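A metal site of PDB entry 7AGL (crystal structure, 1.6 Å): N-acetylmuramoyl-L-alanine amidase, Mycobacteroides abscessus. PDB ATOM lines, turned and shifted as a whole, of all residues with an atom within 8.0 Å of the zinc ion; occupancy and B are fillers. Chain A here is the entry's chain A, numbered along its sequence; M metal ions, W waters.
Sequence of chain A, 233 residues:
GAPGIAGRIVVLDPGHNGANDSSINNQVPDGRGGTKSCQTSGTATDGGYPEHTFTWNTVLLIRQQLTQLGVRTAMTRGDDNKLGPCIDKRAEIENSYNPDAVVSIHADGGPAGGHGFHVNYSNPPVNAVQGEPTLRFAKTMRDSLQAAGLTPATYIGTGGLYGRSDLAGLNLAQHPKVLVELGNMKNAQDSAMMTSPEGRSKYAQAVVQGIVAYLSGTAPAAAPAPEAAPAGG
OE1 of Glu 51 lies close to N of Ala 107, 3.0 Å away. The backbone NH (N) of Glu 51 is in hydrogen-bond range of the backbone carbonyl oxygen (O) of Thr 43 (2.8 Å). O of Glu 51 lies close to OG1 of Thr 55 (3.4 Å). The backbone NH (N) of Glu 51 lies close to the side-chain sulfur (SD) of Met 185 (3.6 Å). N of Gly 42 lies within hydrogen-bond range of ND1 of His 16, at 3.5 Å. NE2 of His 106 sits close to OG of Ser 104 (3.3 Å). The backbone NH (N) of His 106 sits at hydrogen-bond distance from the backbone carbonyl oxygen (O) of Val 180 (2.9 Å). N of Ala 107 lies close to OE1 of Glu 181, 3.1 Å away.
O of Ala 107 touches the zinc ion, 3.9 Å away. The nearest printed residue that does not touch the zinc ion is Glu 181 (4.02 Å).
The zinc ion is bound by OE1 of Glu 51, water W1, NE2 of His 16, ND1 of His 106 and water W2. The zinc ion has five donor atoms within binding distance.
Water W1 bridges the side-chain carboxylate (OE2) of Glu 181 and the backbone carbonyl oxygen (O) of Ala 107.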
ATOM      1  N   PRO A  14     -23.921  -9.994  28.156  1.00  0.00           N
ATOM      2  CA  PRO A  14     -22.479 -10.121  28.342  1.00  0.00           C
ATOM      3  C   PRO A  14     -22.162 -11.425  29.059  1.00  0.00           C
ATOM      4  O   PRO A  14     -22.501 -11.617  30.233  1.00  0.00           O
ATOM      5  CB  PRO A  14     -22.122  -8.888  29.196  1.00  0.00           C
ATOM      6  CG  PRO A  14     -23.406  -8.443  29.850  1.00  0.00           C
ATOM      7  CD  PRO A  14     -24.556  -9.197  29.221  1.00  0.00           C
ATOM      8  N   GLY A  15     -21.506 -12.339  28.331  1.00  0.00           N
ATOM      9  CA  GLY A  15     -21.356 -13.691  28.828  1.00  0.00           C
ATOM     10  C   GLY A  15     -20.586 -13.756  30.143  1.00  0.00           C
ATOM     11  O   GLY A  15     -19.682 -12.961  30.392  1.00  0.00           O
ATOM     12  N   HIS A  16     -20.965 -14.737  30.964  1.00  0.00           N
ATOM     13  CA  HIS A  16     -20.354 -15.080  32.249  1.00  0.00           C
ATOM     14  C   HIS A  16     -20.643 -14.063  33.356  1.00  0.00           C
ATOM     15  O   HIS A  16     -21.280 -13.040  33.123  1.00  0.00           O
ATOM     16  CB  HIS A  16     -18.845 -15.283  32.096  1.00  0.00           C
ATOM     17  CG  HIS A  16     -18.517 -16.256  31.013  1.00  0.00           C
ATOM     18  ND1 HIS A  16     -18.643 -17.625  31.173  1.00  0.00           N
ATOM     19  CD2 HIS A  16     -18.161 -16.054  29.727  1.00  0.00           C
ATOM     20  CE1 HIS A  16     -18.330 -18.231  30.033  1.00  0.00           C
ATOM     21  NE2 HIS A  16     -18.036 -17.295  29.147  1.00  0.00           N
ATOM     22  N   GLN A  39     -23.412 -22.117  35.182  1.00  0.00           N
ATOM     23  CA  GLN A  39     -22.504 -21.141  34.601  1.00  0.00           C
ATOM     24  C   GLN A  39     -21.116 -21.762  34.516  1.00  0.00           C
ATOM     25  O   GLN A  39     -20.840 -22.835  35.074  1.00  0.00           O
ATOM     26  CB  GLN A  39     -22.440 -19.828  35.404  1.00  0.00           C
ATOM     27  CG  GLN A  39     -23.286 -18.671  34.903  1.00  0.00           C
ATOM     28  CD  GLN A  39     -22.943 -18.212  33.484  1.00  0.00           C
ATOM     29  OE1 GLN A  39     -21.916 -18.583  32.914  1.00  0.00           O
ATOM     30  NE2 GLN A  39     -23.830 -17.431  32.905  1.00  0.00           N
ATOM     31  N   THR A  40     -20.260 -21.094  33.744  1.00  0.00           N
ATOM     32  CA  THR A  40     -18.833 -21.364  33.743  1.00  0.00           C
ATOM     33  C   THR A  40     -18.114 -20.039  33.929  1.00  0.00           C
ATOM     34  O   THR A  40     -18.662 -18.966  33.644  1.00  0.00           O
ATOM     35  CB  THR A  40     -18.365 -22.026  32.426  1.00  0.00           C
ATOM     36  OG1 THR A  40     -18.713 -21.167  31.337  1.00  0.00           O
ATOM     37  CG2 THR A  40     -18.999 -23.401  32.221  1.00  0.00           C
ATOM     38  N   SER A  41     -16.874 -20.109  34.405  1.00  0.00           N
ATOM     39  CA  SER A  41     -16.199 -18.860  34.756  1.00  0.00           C
ATOM     40  C   SER A  41     -15.856 -18.044  33.516  1.00  0.00           C
ATOM     41  O   SER A  41     -15.818 -16.806  33.570  1.00  0.00           O
ATOM     42  CB  SER A  41     -14.928 -19.140  35.534  1.00  0.00           C
ATOM     43  OG  SER A  41     -14.030 -19.861  34.724  1.00  0.00           O
ATOM     44  N   GLY A  42     -15.600 -18.702  32.398  1.00  0.00           N
ATOM     45  CA  GLY A  42     -15.102 -18.027  31.216  1.00  0.00           C
ATOM     46  C   GLY A  42     -13.594 -17.919  31.243  1.00  0.00           C
ATOM     47  O   GLY A  42     -12.915 -18.278  32.212  1.00  0.00           O
ATOM     48  N   THR A  43     -13.039 -17.406  30.131  1.00  0.00           N
ATOM     49  CA  THR A  43     -11.597 -17.408  30.000  1.00  0.00           C
ATOM     50  C   THR A  43     -11.046 -16.017  30.349  1.00  0.00           C
ATOM     51  O   THR A  43     -11.702 -15.230  31.052  1.00  0.00           O
ATOM     52  CB  THR A  43     -11.211 -17.909  28.581  1.00  0.00           C
ATOM     53  OG1 THR A  43      -9.799 -18.113  28.509  1.00  0.00           O
ATOM     54  CG2 THR A  43     -11.641 -16.937  27.490  1.00  0.00           C
ATOM     55  N   GLU A  51     -12.560 -12.669  30.517  1.00  0.00           N
ATOM     56  CA  GLU A  51     -13.651 -12.671  29.561  1.00  0.00           C
ATOM     57  C   GLU A  51     -14.862 -11.914  30.085  1.00  0.00           C
ATOM     58  O   GLU A  51     -15.475 -11.115  29.370  1.00  0.00           O
ATOM     59  CB  GLU A  51     -14.056 -14.098  29.211  1.00  0.00           C
ATOM     60  CG  GLU A  51     -15.150 -14.097  28.156  1.00  0.00           C
ATOM     61  CD  GLU A  51     -15.636 -15.478  27.802  1.00  0.00           C
ATOM     62  OE1 GLU A  51     -16.608 -15.540  27.038  1.00  0.00           O
ATOM     63  OE2 GLU A  51     -15.044 -16.487  28.239  1.00  0.00           O
ATOM     64  N   HIS A  52     -15.229 -12.149  31.350  1.00  0.00           N
ATOM     65  CA  HIS A  52     -16.443 -11.522  31.859  1.00  0.00           C
ATOM     66  C   HIS A  52     -16.352 -10.005  31.867  1.00  0.00           C
ATOM     67  O   HIS A  52     -17.369  -9.325  31.687  1.00  0.00           O
ATOM     68  CB  HIS A  52     -16.785 -12.056  33.263  1.00  0.00           C
ATOM     69  CG  HIS A  52     -15.782 -11.751  34.328  1.00  0.00           C
ATOM     70  ND1 HIS A  52     -15.781 -10.565  35.048  1.00  0.00           N
ATOM     71  CD2 HIS A  52     -14.803 -12.511  34.872  1.00  0.00           C
ATOM     72  CE1 HIS A  52     -14.826 -10.622  35.970  1.00  0.00           C
ATOM     73  NE2 HIS A  52     -14.215 -11.779  35.880  1.00  0.00           N
ATOM     74  N   THR A  55     -16.680  -8.833  28.067  1.00  0.00           N
ATOM     75  CA  THR A  55     -18.036  -8.896  27.518  1.00  0.00           C
ATOM     76  C   THR A  55     -18.906  -7.817  28.156  1.00  0.00           C
ATOM     77  O   THR A  55     -19.697  -7.162  27.472  1.00  0.00           O
ATOM     78  CB  THR A  55     -18.655 -10.294  27.711  1.00  0.00           C
ATOM     79  OG1 THR A  55     -18.831 -10.575  29.111  1.00  0.00           O
ATOM     80  CG2 THR A  55     -17.794 -11.406  27.084  1.00  0.00           C
ATOM     81  N   SER A 104     -25.729 -12.343  22.307  1.00  0.00           N
ATOM     82  CA  SER A 104     -24.877 -12.740  23.406  1.00  0.00           C
ATOM     83  C   SER A 104     -23.426 -12.494  22.986  1.00  0.00           C
ATOM     84  O   SER A 104     -23.051 -12.812  21.861  1.00  0.00           O
ATOM     85  CB  SER A 104     -25.114 -14.218  23.741  1.00  0.00           C
ATOM     86  OG  SER A 104     -24.270 -14.684  24.790  1.00  0.00           O
ATOM     87  N   ILE A 105     -22.643 -11.904  23.882  1.00  0.00           N
ATOM     88  CA  ILE A 105     -21.266 -11.487  23.606  1.00  0.00           C
ATOM     89  C   ILE A 105     -20.313 -12.313  24.457  1.00  0.00           C
ATOM     90  O   ILE A 105     -20.436 -12.342  25.697  1.00  0.00           O
ATOM     91  CB  ILE A 105     -21.066  -9.982  23.844  1.00  0.00           C
ATOM     92  CG1 ILE A 105     -21.909  -9.162  22.851  1.00  0.00           C
ATOM     93  CG2 ILE A 105     -19.570  -9.625  23.759  1.00  0.00           C
ATOM     94  CD1 ILE A 105     -21.545  -9.375  21.379  1.00  0.00           C
ATOM     95  N   HIS A 106     -19.354 -12.964  23.795  1.00  0.00           N
ATOM     96  CA  HIS A 106     -18.374 -13.825  24.430  1.00  0.00           C
ATOM     97  C   HIS A 106     -17.003 -13.565  23.803  1.00  0.00           C
ATOM     98  O   HIS A 106     -16.888 -12.873  22.786  1.00  0.00           O
ATOM     99  CB  HIS A 106     -18.762 -15.313  24.261  1.00  0.00           C
ATOM    100  CG  HIS A 106     -19.867 -15.763  25.180  1.00  0.00           C
ATOM    101  ND1 HIS A 106     -19.652 -16.603  26.240  1.00  0.00           N
ATOM    102  CD2 HIS A 106     -21.200 -15.488  25.189  1.00  0.00           C
ATOM    103  CE1 HIS A 106     -20.788 -16.828  26.882  1.00  0.00           C
ATOM    104  NE2 HIS A 106     -21.737 -16.174  26.253  1.00  0.00           N
ATOM    105  N   ALA A 107     -15.962 -14.071  24.455  1.00  0.00           N
ATOM    106  CA  ALA A 107     -14.642 -14.194  23.844  1.00  0.00           C
ATOM    107  C   ALA A 107     -14.071 -15.564  24.202  1.00  0.00           C
ATOM    108  O   ALA A 107     -14.407 -16.143  25.250  1.00  0.00           O
ATOM    109  CB  ALA A 107     -13.686 -13.075  24.275  1.00  0.00           C
ATOM    110  N   ASP A 108     -13.218 -16.073  23.326  1.00  0.00           N
ATOM    111  CA  ASP A 108     -12.911 -17.498  23.280  1.00  0.00           C
ATOM    112  C   ASP A 108     -11.524 -17.772  23.843  1.00  0.00           C
ATOM    113  O   ASP A 108     -10.691 -16.864  23.986  1.00  0.00           O
ATOM    114  CB  ASP A 108     -13.023 -17.989  21.822  1.00  0.00           C
ATOM    115  CG  ASP A 108     -13.175 -19.494  21.692  1.00  0.00           C
ATOM    116  OD1 ASP A 108     -13.533 -20.201  22.673  1.00  0.00           O
ATOM    117  OD2 ASP A 108     -12.933 -19.968  20.549  1.00  0.00           O
ATOM    118  N   GLY A 109     -11.276 -19.050  24.152  1.00  0.00           N
ATOM    119  CA  GLY A 109      -9.943 -19.517  24.459  1.00  0.00           C
ATOM    120  C   GLY A 109      -9.568 -20.597  23.463  1.00  0.00           C
ATOM    121  O   GLY A 109     -10.065 -21.726  23.559  1.00  0.00           O
ATOM    122  N   LEU A 179     -24.882 -15.813  19.260  1.00  0.00           N
ATOM    123  CA  LEU A 179     -23.842 -15.697  20.271  1.00  0.00           C
ATOM    124  C   LEU A 179     -22.558 -15.412  19.514  1.00  0.00           C
ATOM    125  O   LEU A 179     -22.077 -16.286  18.777  1.00  0.00           O
ATOM    126  CB  LEU A 179     -23.725 -16.968  21.120  1.00  0.00           C
ATOM    127  CG  LEU A 179     -22.773 -16.944  22.330  1.00  0.00           C
ATOM    128  CD1 LEU A 179     -23.090 -18.125  23.259  1.00  0.00           C
ATOM    129  CD2 LEU A 179     -21.278 -16.964  21.965  1.00  0.00           C
ATOM    130  N   VAL A 180     -22.029 -14.203  19.667  1.00  0.00           N
ATOM    131  CA  VAL A 180     -20.844 -13.782  18.928  1.00  0.00           C
ATOM    132  C   VAL A 180     -19.638 -13.970  19.840  1.00  0.00           C
ATOM    133  O   VAL A 180     -19.540 -13.311  20.873  1.00  0.00           O
ATOM    134  CB  VAL A 180     -20.948 -12.323  18.460  1.00  0.00           C
ATOM    135  CG1 VAL A 180     -19.716 -11.964  17.620  1.00  0.00           C
ATOM    136  CG2 VAL A 180     -22.222 -12.126  17.632  1.00  0.00           C
ATOM    137  N   GLU A 181     -18.745 -14.875  19.453  1.00  0.00           N
ATOM    138  CA  GLU A 181     -17.405 -14.940  20.026  1.00  0.00           C
ATOM    139  C   GLU A 181     -16.543 -13.951  19.241  1.00  0.00           C
ATOM    140  O   GLU A 181     -16.266 -14.161  18.052  1.00  0.00           O
ATOM    141  CB  GLU A 181     -16.857 -16.364  19.958  1.00  0.00           C
ATOM    142  CG  GLU A 181     -17.596 -17.371  20.879  1.00  0.00           C
ATOM    143  CD  GLU A 181     -17.036 -17.405  22.278  1.00  0.00           C
ATOM    144  OE1 GLU A 181     -16.159 -16.553  22.561  1.00  0.00           O
ATOM    145  OE2 GLU A 181     -17.468 -18.269  23.089  1.00  0.00           O
ATOM    146  N   MET A 185      -9.113 -14.803  23.206  1.00  0.00           N
ATOM    147  CA  MET A 185      -8.370 -14.066  24.246  1.00  0.00           C
ATOM    148  C   MET A 185      -6.937 -14.551  24.393  1.00  0.00           C
ATOM    149  O   MET A 185      -6.095 -13.812  24.935  1.00  0.00           O
ATOM    150  CB  MET A 185      -9.073 -14.191  25.613  1.00  0.00           C
ATOM    151  CG  MET A 185     -10.540 -13.830  25.593  1.00  0.00           C
ATOM    152  SD  MET A 185     -11.168 -13.352  27.226  1.00  0.00           S
ATOM    153  CE  MET A 185     -10.828 -11.596  27.174  1.00  0.00           C
HETATM  154 ZN    ZN M   1     -17.738 -17.327  26.990  1.00  0.00          ZN
HETATM  155  O   HOH W   1     -16.479 -17.989  25.351  1.00  0.00           O
HETATM  156  O   HOH W   2     -18.323 -19.494  27.039  1.00  0.00           O
